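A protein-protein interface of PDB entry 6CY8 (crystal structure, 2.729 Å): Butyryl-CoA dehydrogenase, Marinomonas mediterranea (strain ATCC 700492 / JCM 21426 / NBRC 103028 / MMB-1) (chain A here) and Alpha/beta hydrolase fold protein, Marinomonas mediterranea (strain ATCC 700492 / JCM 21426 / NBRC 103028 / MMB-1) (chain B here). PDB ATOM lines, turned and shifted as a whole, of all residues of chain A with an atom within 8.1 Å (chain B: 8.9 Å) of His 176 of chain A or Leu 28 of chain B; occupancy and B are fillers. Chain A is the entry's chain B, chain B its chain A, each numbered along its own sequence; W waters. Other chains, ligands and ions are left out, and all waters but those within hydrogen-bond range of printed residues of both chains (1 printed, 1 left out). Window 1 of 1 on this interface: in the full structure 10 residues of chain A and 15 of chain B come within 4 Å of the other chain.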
ATOM      1  N   SER A 135      25.060   9.583  -7.971  1.00  0.00           N
ATOM      2  CA  SER A 135      24.291  10.781  -8.273  1.00  0.00           C
ATOM      3  C   SER A 135      25.122  12.047  -8.153  1.00  0.00           C
ATOM      4  O   SER A 135      24.797  13.056  -8.794  1.00  0.00           O
ATOM      5  CB  SER A 135      23.079  10.888  -7.328  1.00  0.00           C
ATOM      6  OG  SER A 135      23.492  11.057  -5.964  1.00  0.00           O
ATOM      7  N   THR A 171      31.082  14.652 -13.817  1.00  0.00           N
ATOM      8  CA  THR A 171      30.099  15.713 -13.661  1.00  0.00           C
ATOM      9  C   THR A 171      30.464  16.872 -14.582  1.00  0.00           C
ATOM     10  O   THR A 171      31.566  17.422 -14.495  1.00  0.00           O
ATOM     11  CB  THR A 171      30.047  16.179 -12.211  1.00  0.00           C
ATOM     12  OG1 THR A 171      29.880  15.051 -11.341  1.00  0.00           O
ATOM     13  CG2 THR A 171      28.885  17.150 -12.017  1.00  0.00           C
ATOM     14  N   THR A 172      29.551  17.245 -15.470  1.00  0.00           N
ATOM     15  CA  THR A 172      29.797  18.387 -16.331  1.00  0.00           C
ATOM     16  C   THR A 172      29.023  19.629 -15.909  1.00  0.00           C
ATOM     17  O   THR A 172      29.364  20.731 -16.356  1.00  0.00           O
ATOM     18  CB  THR A 172      29.454  18.036 -17.771  1.00  0.00           C
ATOM     19  OG1 THR A 172      28.256  17.250 -17.798  1.00  0.00           O
ATOM     20  CG2 THR A 172      30.607  17.266 -18.396  1.00  0.00           C
ATOM     21  N   ASN A 173      28.032  19.475 -15.027  1.00  0.00           N
ATOM     22  CA  ASN A 173      27.074  20.515 -14.682  1.00  0.00           C
ATOM     23  C   ASN A 173      26.341  20.135 -13.400  1.00  0.00           C
ATOM     24  O   ASN A 173      25.284  19.499 -13.449  1.00  0.00           O
ATOM     25  CB  ASN A 173      26.079  20.714 -15.825  1.00  0.00           C
ATOM     26  CG  ASN A 173      25.361  22.055 -15.756  1.00  0.00           C
ATOM     27  OD1 ASN A 173      25.146  22.614 -14.672  1.00  0.00           O
ATOM     28  ND2 ASN A 173      24.988  22.581 -16.926  1.00  0.00           N
ATOM     29  N   LYS A 174      26.896  20.518 -12.247  1.00  0.00           N
ATOM     30  CA  LYS A 174      26.336  20.083 -10.971  1.00  0.00           C
ATOM     31  C   LYS A 174      24.873  20.490 -10.792  1.00  0.00           C
ATOM     32  O   LYS A 174      24.152  19.838 -10.029  1.00  0.00           O
ATOM     33  CB  LYS A 174      27.196  20.617  -9.817  1.00  0.00           C
ATOM     34  CG  LYS A 174      26.964  19.901  -8.488  1.00  0.00           C
ATOM     35  CD  LYS A 174      27.821  20.457  -7.350  1.00  0.00           C
ATOM     36  CE  LYS A 174      29.115  19.660  -7.159  1.00  0.00           C
ATOM     37  NZ  LYS A 174      29.301  19.140  -5.757  1.00  0.00           N
ATOM     38  N   LYS A 175      24.421  21.514 -11.490  1.00  0.00           N
ATOM     39  CA  LYS A 175      23.063  21.997 -11.328  1.00  0.00           C
ATOM     40  C   LYS A 175      22.001  21.168 -12.011  1.00  0.00           C
ATOM     41  O   LYS A 175      20.850  21.233 -11.662  1.00  0.00           O
ATOM     42  CB  LYS A 175      22.964  23.446 -11.786  1.00  0.00           C
ATOM     43  N   HIS A 176      22.384  20.420 -13.019  1.00  0.00           N
ATOM     44  CA  HIS A 176      21.447  19.552 -13.719  1.00  0.00           C
ATOM     45  C   HIS A 176      21.329  18.162 -13.076  1.00  0.00           C
ATOM     46  O   HIS A 176      20.641  17.292 -13.629  1.00  0.00           O
ATOM     47  CB  HIS A 176      21.852  19.444 -15.192  1.00  0.00           C
ATOM     48  CG  HIS A 176      21.737  20.737 -15.943  1.00  0.00           C
ATOM     49  ND1 HIS A 176      22.289  20.929 -17.192  1.00  0.00           N
ATOM     50  CD2 HIS A 176      21.131  21.904 -15.619  1.00  0.00           C
ATOM     51  CE1 HIS A 176      22.027  22.156 -17.603  1.00  0.00           C
ATOM     52  NE2 HIS A 176      21.327  22.768 -16.667  1.00  0.00           N
ATOM     53  N   GLY A 177      21.982  17.947 -11.929  1.00  0.00           N
ATOM     54  CA  GLY A 177      21.915  16.721 -11.151  1.00  0.00           C
ATOM     55  C   GLY A 177      22.040  15.409 -11.906  1.00  0.00           C
ATOM     56  O   GLY A 177      23.035  15.148 -12.591  1.00  0.00           O
ATOM     57  N   TYR A 178      21.007  14.573 -11.775  1.00  0.00           N
ATOM     58  CA  TYR A 178      20.941  13.304 -12.487  1.00  0.00           C
ATOM     59  C   TYR A 178      21.252  13.463 -13.968  1.00  0.00           C
ATOM     60  O   TYR A 178      21.689  12.498 -14.610  1.00  0.00           O
ATOM     61  CB  TYR A 178      19.551  12.696 -12.239  1.00  0.00           C
ATOM     62  CG  TYR A 178      19.031  11.652 -13.212  1.00  0.00           C
ATOM     63  CD1 TYR A 178      19.650  10.409 -13.347  1.00  0.00           C
ATOM     64  CD2 TYR A 178      17.867  11.890 -13.943  1.00  0.00           C
ATOM     65  CE1 TYR A 178      19.147   9.445 -14.227  1.00  0.00           C
ATOM     66  CE2 TYR A 178      17.354  10.943 -14.821  1.00  0.00           C
ATOM     67  CZ  TYR A 178      17.994   9.720 -14.960  1.00  0.00           C
ATOM     68  OH  TYR A 178      17.477   8.783 -15.837  1.00  0.00           O
ATOM     69  N   LEU A 179      21.084  14.664 -14.523  1.00  0.00           N
ATOM     70  CA  LEU A 179      21.377  14.907 -15.931  1.00  0.00           C
ATOM     71  C   LEU A 179      22.622  15.774 -16.142  1.00  0.00           C
ATOM     72  O   LEU A 179      22.852  16.244 -17.260  1.00  0.00           O
ATOM     73  CB  LEU A 179      20.157  15.523 -16.611  1.00  0.00           C
ATOM     74  CG  LEU A 179      18.932  14.598 -16.576  1.00  0.00           C
ATOM     75  CD1 LEU A 179      17.794  15.117 -17.443  1.00  0.00           C
ATOM     76  CD2 LEU A 179      19.307  13.186 -17.004  1.00  0.00           C
ATOM     77  N   GLY A 180      23.447  15.963 -15.105  1.00  0.00           N
ATOM     78  CA  GLY A 180      24.643  16.790 -15.198  1.00  0.00           C
ATOM     79  C   GLY A 180      25.958  16.040 -15.371  1.00  0.00           C
ATOM     80  O   GLY A 180      27.021  16.509 -14.931  1.00  0.00           O
ATOM     81  N   GLN A 181      25.900  14.883 -16.035  1.00  0.00           N
ATOM     82  CA  GLN A 181      27.010  13.952 -16.093  1.00  0.00           C
ATOM     83  C   GLN A 181      27.222  13.512 -17.530  1.00  0.00           C
ATOM     84  O   GLN A 181      26.258  13.248 -18.247  1.00  0.00           O
ATOM     85  CB  GLN A 181      26.742  12.723 -15.209  1.00  0.00           C
ATOM     86  CG  GLN A 181      26.508  13.024 -13.742  1.00  0.00           C
ATOM     87  CD  GLN A 181      26.201  11.773 -12.946  1.00  0.00           C
ATOM     88  OE1 GLN A 181      26.040  10.691 -13.522  1.00  0.00           O
ATOM     89  NE2 GLN A 181      26.130  11.906 -11.613  1.00  0.00           N
ATOM     90  N   GLU A 228      26.384  15.749 -24.047  1.00  0.00           N
ATOM     91  CA  GLU A 228      26.717  16.135 -22.684  1.00  0.00           C
ATOM     92  C   GLU A 228      25.474  16.029 -21.809  1.00  0.00           C
ATOM     93  O   GLU A 228      24.360  16.342 -22.243  1.00  0.00           O
ATOM     94  CB  GLU A 228      27.269  17.561 -22.660  1.00  0.00           C
ATOM     95  CG  GLU A 228      27.651  18.077 -21.271  1.00  0.00           C
ATOM     96  CD  GLU A 228      26.500  18.797 -20.576  1.00  0.00           C
ATOM     97  OE1 GLU A 228      26.520  18.930 -19.318  1.00  0.00           O
ATOM     98  OE2 GLU A 228      25.571  19.222 -21.305  1.00  0.00           O
ATOM     99  N   GLY A 229      25.663  15.573 -20.571  1.00  0.00           N
ATOM    100  CA  GLY A 229      24.557  15.396 -19.647  1.00  0.00           C
ATOM    101  C   GLY A 229      23.814  14.074 -19.754  1.00  0.00           C
ATOM    102  O   GLY A 229      22.925  13.815 -18.935  1.00  0.00           O
ATOM    103  N   ASN B  24       8.053  26.298 -10.160  1.00  0.00           N
ATOM    104  CA  ASN B  24       9.396  26.849 -10.268  1.00  0.00           C
ATOM    105  C   ASN B  24      10.404  26.169  -9.366  1.00  0.00           C
ATOM    106  O   ASN B  24      11.582  26.548  -9.382  1.00  0.00           O
ATOM    107  CB  ASN B  24       9.382  28.343  -9.959  1.00  0.00           C
ATOM    108  CG  ASN B  24       8.683  29.122 -11.017  1.00  0.00           C
ATOM    109  OD1 ASN B  24       7.663  29.757 -10.767  1.00  0.00           O
ATOM    110  ND2 ASN B  24       9.210  29.046 -12.242  1.00  0.00           N
ATOM    111  N   THR B  25       9.977  25.206  -8.571  1.00  0.00           N
ATOM    112  CA  THR B  25      10.926  24.418  -7.810  1.00  0.00           C
ATOM    113  C   THR B  25      11.829  23.657  -8.782  1.00  0.00           C
ATOM    114  O   THR B  25      11.328  23.004  -9.712  1.00  0.00           O
ATOM    115  CB  THR B  25      10.175  23.481  -6.862  1.00  0.00           C
ATOM    116  OG1 THR B  25       9.017  24.158  -6.350  1.00  0.00           O
ATOM    117  CG2 THR B  25      11.052  23.056  -5.690  1.00  0.00           C
ATOM    118  N   PRO B  26      13.156  23.773  -8.650  1.00  0.00           N
ATOM    119  CA  PRO B  26      14.086  23.121  -9.591  1.00  0.00           C
ATOM    120  C   PRO B  26      14.215  21.623  -9.327  1.00  0.00           C
ATOM    121  O   PRO B  26      14.875  21.192  -8.372  1.00  0.00           O
ATOM    122  CB  PRO B  26      15.406  23.869  -9.345  1.00  0.00           C
ATOM    123  CG  PRO B  26      15.291  24.406  -7.945  1.00  0.00           C
ATOM    124  CD  PRO B  26      13.840  24.671  -7.698  1.00  0.00           C
ATOM    125  N   LEU B  27      13.598  20.819 -10.198  1.00  0.00           N
ATOM    126  CA  LEU B  27      13.502  19.373  -9.978  1.00  0.00           C
ATOM    127  C   LEU B  27      14.872  18.703 -10.007  1.00  0.00           C
ATOM    128  O   LEU B  27      15.208  17.922  -9.110  1.00  0.00           O
ATOM    129  CB  LEU B  27      12.579  18.744 -11.025  1.00  0.00           C
ATOM    130  CG  LEU B  27      11.136  19.255 -11.053  1.00  0.00           C
ATOM    131  CD1 LEU B  27      10.338  18.660 -12.222  1.00  0.00           C
ATOM    132  CD2 LEU B  27      10.438  19.019  -9.715  1.00  0.00           C
ATOM    133  N   LEU B  28      15.676  18.986 -11.036  1.00  0.00           N
ATOM    134  CA  LEU B  28      16.992  18.366 -11.138  1.00  0.00           C
ATOM    135  C   LEU B  28      17.957  18.920 -10.099  1.00  0.00           C
ATOM    136  O   LEU B  28      18.698  18.158  -9.469  1.00  0.00           O
ATOM    137  CB  LEU B  28      17.548  18.555 -12.544  1.00  0.00           C
ATOM    138  CG  LEU B  28      16.650  17.962 -13.632  1.00  0.00           C
ATOM    139  CD1 LEU B  28      17.085  18.359 -15.037  1.00  0.00           C
ATOM    140  CD2 LEU B  28      16.582  16.445 -13.498  1.00  0.00           C
ATOM    141  N   GLU B  29      17.967  20.237  -9.898  1.00  0.00           N
ATOM    142  CA  GLU B  29      18.991  20.830  -9.039  1.00  0.00           C
ATOM    143  C   GLU B  29      18.858  20.355  -7.593  1.00  0.00           C
ATOM    144  O   GLU B  29      19.869  20.143  -6.911  1.00  0.00           O
ATOM    145  CB  GLU B  29      18.932  22.357  -9.107  1.00  0.00           C
ATOM    146  CG  GLU B  29      19.785  23.073  -8.045  1.00  0.00           C
ATOM    147  CD  GLU B  29      20.163  24.498  -8.441  1.00  0.00           C
ATOM    148  OE1 GLU B  29      19.635  25.005  -9.459  1.00  0.00           O
ATOM    149  OE2 GLU B  29      20.989  25.113  -7.725  1.00  0.00           O
ATOM    150  N   LEU B  30      17.634  20.181  -7.101  1.00  0.00           N
ATOM    151  CA  LEU B  30      17.458  19.816  -5.703  1.00  0.00           C
ATOM    152  C   LEU B  30      17.232  18.322  -5.494  1.00  0.00           C
ATOM    153  O   LEU B  30      17.051  17.893  -4.351  1.00  0.00           O
ATOM    154  CB  LEU B  30      16.312  20.619  -5.070  1.00  0.00           C
ATOM    155  CG  LEU B  30      16.588  22.102  -4.790  1.00  0.00           C
ATOM    156  CD1 LEU B  30      15.273  22.824  -4.499  1.00  0.00           C
ATOM    157  CD2 LEU B  30      17.613  22.335  -3.659  1.00  0.00           C
ATOM    158  N   GLY B  31      17.262  17.524  -6.556  1.00  0.00           N
ATOM    159  CA  GLY B  31      17.301  16.082  -6.445  1.00  0.00           C
ATOM    160  C   GLY B  31      15.972  15.368  -6.540  1.00  0.00           C
ATOM    161  O   GLY B  31      15.930  14.153  -6.313  1.00  0.00           O
ATOM    162  N   ILE B  32      14.891  16.075  -6.871  1.00  0.00           N
ATOM    163  CA  ILE B  32      13.570  15.461  -6.861  1.00  0.00           C
ATOM    164  C   ILE B  32      13.447  14.417  -7.967  1.00  0.00           C
ATOM    165  O   ILE B  32      12.881  13.336  -7.753  1.00  0.00           O
ATOM    166  CB  ILE B  32      12.485  16.544  -6.969  1.00  0.00           C
ATOM    167  CG1 ILE B  32      12.373  17.297  -5.647  1.00  0.00           C
ATOM    168  CG2 ILE B  32      11.144  15.941  -7.379  1.00  0.00           C
ATOM    169  CD1 ILE B  32      11.803  18.685  -5.802  1.00  0.00           C
ATOM    170  N   LEU B  33      13.964  14.705  -9.163  1.00  0.00           N
ATOM    171  CA  LEU B  33      14.025  13.687 -10.202  1.00  0.00           C
ATOM    172  C   LEU B  33      15.424  13.106 -10.263  1.00  0.00           C
ATOM    173  O   LEU B  33      16.385  13.786 -10.637  1.00  0.00           O
ATOM    174  CB  LEU B  33      13.603  14.189 -11.575  1.00  0.00           C
ATOM    175  CG  LEU B  33      12.213  14.771 -11.649  1.00  0.00           C
ATOM    176  CD1 LEU B  33      12.147  15.720 -12.835  1.00  0.00           C
ATOM    177  CD2 LEU B  33      11.202  13.631 -11.764  1.00  0.00           C
ATOM    178  N   ASP B  34      15.510  11.839  -9.922  1.00  0.00           N
ATOM    179  CA  ASP B  34      16.674  11.025 -10.124  1.00  0.00           C
ATOM    180  C   ASP B  34      16.299   9.854 -11.013  1.00  0.00           C
ATOM    181  O   ASP B  34      15.184   9.747 -11.529  1.00  0.00           O
ATOM    182  CB  ASP B  34      17.221  10.528  -8.789  1.00  0.00           C
ATOM    183  CG  ASP B  34      16.121   9.962  -7.878  1.00  0.00           C
ATOM    184  OD1 ASP B  34      15.502   8.932  -8.245  1.00  0.00           O
ATOM    185  OD2 ASP B  34      15.878  10.544  -6.791  1.00  0.00           O
ATOM    186  N   SER B  35      17.185   8.885 -10.991  1.00  0.00           N
ATOM    187  CA  SER B  35      17.036   7.633 -11.698  1.00  0.00           C
ATOM    188  C   SER B  35      15.786   6.900 -11.345  1.00  0.00           C
ATOM    189  O   SER B  35      15.156   6.384 -12.225  1.00  0.00           O
ATOM    190  CB  SER B  35      18.203   6.711 -11.423  1.00  0.00           C
ATOM    191  N   SER B  37      12.884   8.121  -9.461  1.00  0.00           N
ATOM    192  CA  SER B  37      11.705   8.968  -9.613  1.00  0.00           C
ATOM    193  C   SER B  37      11.371   9.223 -11.077  1.00  0.00           C
ATOM    194  O   SER B  37      10.191   9.363 -11.422  1.00  0.00           O
ATOM    195  CB  SER B  37      11.922  10.282  -8.883  1.00  0.00           C
ATOM    196  OG  SER B  37      13.187  10.789  -9.237  1.00  0.00           O
ATOM    197  N   MET B  38      12.380   9.274 -11.946  1.00  0.00           N
ATOM    198  CA  MET B  38      12.112   9.453 -13.368  1.00  0.00           C
ATOM    199  C   MET B  38      11.211   8.347 -13.908  1.00  0.00           C
ATOM    200  O   MET B  38      10.259   8.614 -14.652  1.00  0.00           O
ATOM    201  CB  MET B  38      13.429   9.493 -14.141  1.00  0.00           C
ATOM    202  CG  MET B  38      13.264   9.769 -15.636  1.00  0.00           C
ATOM    203  SD  MET B  38      12.524  11.386 -15.970  1.00  0.00           S
ATOM    204  CE  MET B  38      13.515  12.472 -14.933  1.00  0.00           C
ATOM    205  N   LEU B  41       7.732   8.914 -12.852  1.00  0.00           N
ATOM    206  CA  LEU B  41       7.176  10.041 -13.586  1.00  0.00           C
ATOM    207  C   LEU B  41       6.861   9.657 -15.027  1.00  0.00           C
ATOM    208  O   LEU B  41       5.749   9.899 -15.515  1.00  0.00           O
ATOM    209  CB  LEU B  41       8.146  11.214 -13.534  1.00  0.00           C
ATOM    210  CG  LEU B  41       7.662  12.533 -14.131  1.00  0.00           C
ATOM    211  CD1 LEU B  41       6.887  13.338 -13.094  1.00  0.00           C
ATOM    212  CD2 LEU B  41       8.845  13.336 -14.663  1.00  0.00           C
ATOM    213  N   ILE B  58      14.716  13.659 -22.973  1.00  0.00           N
ATOM    214  CA  ILE B  58      15.103  13.721 -21.566  1.00  0.00           C
ATOM    215  C   ILE B  58      16.373  14.565 -21.471  1.00  0.00           C
ATOM    216  O   ILE B  58      17.453  14.112 -21.858  1.00  0.00           O
ATOM    217  CB  ILE B  58      15.327  12.329 -20.968  1.00  0.00           C
ATOM    218  CG1 ILE B  58      14.027  11.530 -20.961  1.00  0.00           C
ATOM    219  CG2 ILE B  58      15.878  12.446 -19.554  1.00  0.00           C
ATOM    220  CD1 ILE B  58      13.997  10.438 -21.966  1.00  0.00           C
ATOM    221  N   ASN B  59      16.253  15.784 -20.957  1.00  0.00           N
ATOM    222  CA  ASN B  59      17.366  16.730 -20.927  1.00  0.00           C
ATOM    223  C   ASN B  59      17.059  17.784 -19.866  1.00  0.00           C
ATOM    224  O   ASN B  59      15.928  17.873 -19.380  1.00  0.00           O
ATOM    225  CB  ASN B  59      17.606  17.356 -22.319  1.00  0.00           C
ATOM    226  CG  ASN B  59      16.461  18.241 -22.785  1.00  0.00           C
ATOM    227  OD1 ASN B  59      16.067  19.202 -22.110  1.00  0.00           O
ATOM    228  ND2 ASN B  59      15.917  17.915 -23.954  1.00  0.00           N
ATOM    229  N   PRO B  60      18.065  18.577 -19.458  1.00  0.00           N
ATOM    230  CA  PRO B  60      17.849  19.539 -18.355  1.00  0.00           C
ATOM    231  C   PRO B  60      16.992  20.746 -18.709  1.00  0.00           C
ATOM    232  O   PRO B  60      16.478  21.408 -17.793  1.00  0.00           O
ATOM    233  CB  PRO B  60      19.275  19.992 -17.996  1.00  0.00           C
ATOM    234  CG  PRO B  60      20.184  19.010 -18.639  1.00  0.00           C
ATOM    235  CD  PRO B  60      19.478  18.509 -19.845  1.00  0.00           C
ATOM    236  N   GLU B  61      16.868  21.080 -19.996  1.00  0.00           N
ATOM    237  CA  GLU B  61      15.927  22.102 -20.440  1.00  0.00           C
ATOM    238  C   GLU B  61      14.503  21.727 -20.065  1.00  0.00           C
ATOM    239  O   GLU B  61      13.818  22.451 -19.330  1.00  0.00           O
ATOM    240  CB  GLU B  61      16.020  22.271 -21.957  1.00  0.00           C
ATOM    241  CG  GLU B  61      15.352  23.511 -22.509  1.00  0.00           C
ATOM    242  CD  GLU B  61      16.048  24.012 -23.745  1.00  0.00           C
ATOM    243  OE1 GLU B  61      15.876  23.383 -24.812  1.00  0.00           O
ATOM    244  OE2 GLU B  61      16.788  25.016 -23.656  1.00  0.00           O
ATOM    245  N   HIS B  62      14.040  20.589 -20.593  1.00  0.00           N
ATOM    246  CA  HIS B  62      12.652  20.190 -20.421  1.00  0.00           C
ATOM    247  C   HIS B  62      12.338  19.774 -18.993  1.00  0.00           C
ATOM    248  O   HIS B  62      11.211  19.980 -18.534  1.00  0.00           O
ATOM    249  CB  HIS B  62      12.317  19.064 -21.392  1.00  0.00           C
ATOM    250  CG  HIS B  62      12.496  19.458 -22.823  1.00  0.00           C
ATOM    251  ND1 HIS B  62      12.595  20.775 -23.218  1.00  0.00           N
ATOM    252  CD2 HIS B  62      12.588  18.719 -23.951  1.00  0.00           C
ATOM    253  CE1 HIS B  62      12.744  20.828 -24.530  1.00  0.00           C
ATOM    254  NE2 HIS B  62      12.739  19.593 -25.000  1.00  0.00           N
ATOM    255  N   PHE B  63      13.302  19.208 -18.269  1.00  0.00           N
ATOM    256  CA  PHE B  63      13.060  18.726 -16.918  1.00  0.00           C
ATOM    257  C   PHE B  63      13.615  19.678 -15.875  1.00  0.00           C
ATOM    258  O   PHE B  63      13.840  19.283 -14.727  1.00  0.00           O
ATOM    259  CB  PHE B  63      13.623  17.309 -16.753  1.00  0.00           C
ATOM    260  CG  PHE B  63      12.847  16.261 -17.526  1.00  0.00           C
ATOM    261  CD1 PHE B  63      13.123  16.022 -18.865  1.00  0.00           C
ATOM    262  CD2 PHE B  63      11.811  15.552 -16.929  1.00  0.00           C
ATOM    263  CE1 PHE B  63      12.399  15.072 -19.592  1.00  0.00           C
ATOM    264  CE2 PHE B  63      11.081  14.607 -17.657  1.00  0.00           C
ATOM    265  CZ  PHE B  63      11.378  14.371 -18.994  1.00  0.00           C
ATOM    266  N   GLU B  64      13.831  20.932 -16.256  1.00  0.00           N
ATOM    267  CA  GLU B  64      14.257  21.944 -15.296  1.00  0.00           C
ATOM    268  C   GLU B  64      13.257  22.074 -14.153  1.00  0.00           C
ATOM    269  O   GLU B  64      13.647  22.165 -12.982  1.00  0.00           O
ATOM    270  CB  GLU B  64      14.432  23.271 -16.027  1.00  0.00           C
ATOM    271  CG  GLU B  64      14.922  24.445 -15.204  1.00  0.00           C
ATOM    272  CD  GLU B  64      15.158  25.647 -16.094  1.00  0.00           C
ATOM    273  OE1 GLU B  64      14.873  25.535 -17.315  1.00  0.00           O
ATOM    274  OE2 GLU B  64      15.620  26.688 -15.583  1.00  0.00           O
ATOM    275  N   ASN B  65      11.963  22.073 -14.474  1.00  0.00           N
ATOM    276  CA  ASN B  65      10.903  22.177 -13.476  1.00  0.00           C
ATOM    277  C   ASN B  65       9.593  21.725 -14.108  1.00  0.00           C
ATOM    278  O   ASN B  65       9.546  21.327 -15.278  1.00  0.00           O
ATOM    279  CB  ASN B  65      10.783  23.600 -12.914  1.00  0.00           C
ATOM    280  CG  ASN B  65      10.895  24.683 -13.997  1.00  0.00           C
ATOM    281  OD1 ASN B  65      10.235  24.623 -15.052  1.00  0.00           O
ATOM    282  ND2 ASN B  65      11.738  25.684 -13.729  1.00  0.00           N
ATOM    283  N   VAL B  66       8.521  21.808 -13.305  1.00  0.00           N
ATOM    284  CA  VAL B  66       7.200  21.319 -13.700  1.00  0.00           C
ATOM    285  C   VAL B  66       6.687  22.083 -14.912  1.00  0.00           C
ATOM    286  O   VAL B  66       6.096  21.503 -15.838  1.00  0.00           O
ATOM    287  CB  VAL B  66       6.223  21.442 -12.513  1.00  0.00           C
ATOM    288  CG1 VAL B  66       5.032  20.494 -12.679  1.00  0.00           C
ATOM    289  CG2 VAL B  66       6.947  21.235 -11.181  1.00  0.00           C
ATOM    290  N   THR B  68       8.434  23.769 -17.356  1.00  0.00           N
ATOM    291  CA  THR B  68       9.140  23.305 -18.550  1.00  0.00           C
ATOM    292  C   THR B  68       8.740  21.880 -18.905  1.00  0.00           C
ATOM    293  O   THR B  68       8.615  21.534 -20.087  1.00  0.00           O
ATOM    294  CB  THR B  68      10.654  23.379 -18.340  1.00  0.00           C
ATOM    295  OG1 THR B  68      11.005  22.713 -17.118  1.00  0.00           O
ATOM    296  CG2 THR B  68      11.130  24.826 -18.275  1.00  0.00           C
HETATM  297  O   HOH W   1      18.350  15.353 -10.177  1.00  0.00           O
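The side-chain amide oxygen (OD1) of Asn 173 of chain A lies close to the backbone NH (N) of Lys 175 of chain A, 3.4 Å away.
ND2 of Asn 173 of chain A lies close to ND1 of His 176 of chain A (3.2 Å).
O of Leu 27 of chain B lies within hydrogen-bond range of N of Leu 33 of chain B.
The side-chain hydroxyl (OG) of Ser 37 of chain B sits at hydrogen-bond distance from the backbone NH (N) of Asp 34 of chain B, 2.6 Å away.
The backbone NH (N) of Glu 61 of chain B is in hydrogen-bond range of the side-chain amide oxygen (OD1) of Asn 59 of chain B.
The side-chain amide oxygen (OD1) of Asn 59 of chain B sits at hydrogen-bond distance from the backbone NH (N) of His 62 of chain B (2.9 Å).
Lys 175 of chain A touches Glu 29 of chain B (O to CA, 3.2 Å).
His 176 of chain A touches Leu 28 of chain B (O to CB, 3.5 Å).
His 176 of chain A touches Pro 60 of chain B.
Gly 177 of chain A touches Leu 28 of chain B.
O of Leu 33 of chain B touches CB of Tyr 178 of chain A, at 3.7 Å.
Asp 34 of chain B touches Tyr 178 of chain A (C to CD2, 3.9 Å).
CD1 of Tyr 178 of chain A touches N of Ser 35 of chain B, at 3.7 Å.
CD1 of Leu 179 of chain A touches CG2 of Ile 58 of chain B, 3.9 Å away.
CD1 of Leu 179 of chain A touches C of Asn 59 of chain B (3.7 Å).
His 176 of chain A touches two residues of chain B.
Gly 177 of chain A touches just one residue of chain B: Leu 28 (3.9 Å).
Leu 27 of chain B touches none of the printed residues of chain A.
Leu 28 of chain B touches two residues of chain A.
Of the printed residues of chain A, Ser 35 of chain B touches Tyr 178 (3.7 Å).
Of the printed residues of chain A, Asn 59 of chain B touches Leu 179.
Of the printed residues of chain A, Pro 60 of chain B touches His 176 (3.2 Å).
The nearest residue of chain B that does not touch His 176 of chain A is Glu 29 of chain B (5.1 Å).
The nearest residue of chain A that does not touch Leu 28 of chain B is Lys 175 of chain A (4.02 Å).
The nearest printed residue of chain B that does not touch Tyr 178 of chain A is Met 38 of chain B (4.1 Å).
Hydrophobic or aromatic side chains of chain A that line the printed part of chain B: His 176, Tyr 178 and Leu 179.
Hydrophobic or aromatic side chains of chain B that line the printed part of chain A: Leu 28, Ile 58 and Pro 60.
Among the printed residues, 9 pairs touch across the chains.
Among the printed residues, no Asp or Glu carboxylate lies within 4 Å of a Lys or Arg side-chain nitrogen of the other chain.
Water W1 lies within hydrogen-bond range of the backbone carbonyl oxygen of Leu 33 of chain B (2.6 Å), the backbone carbonyl oxygen of Leu 28 of chain B (2.9 Å) and the backbone NH of Tyr 178 of chain A (3.2 Å).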
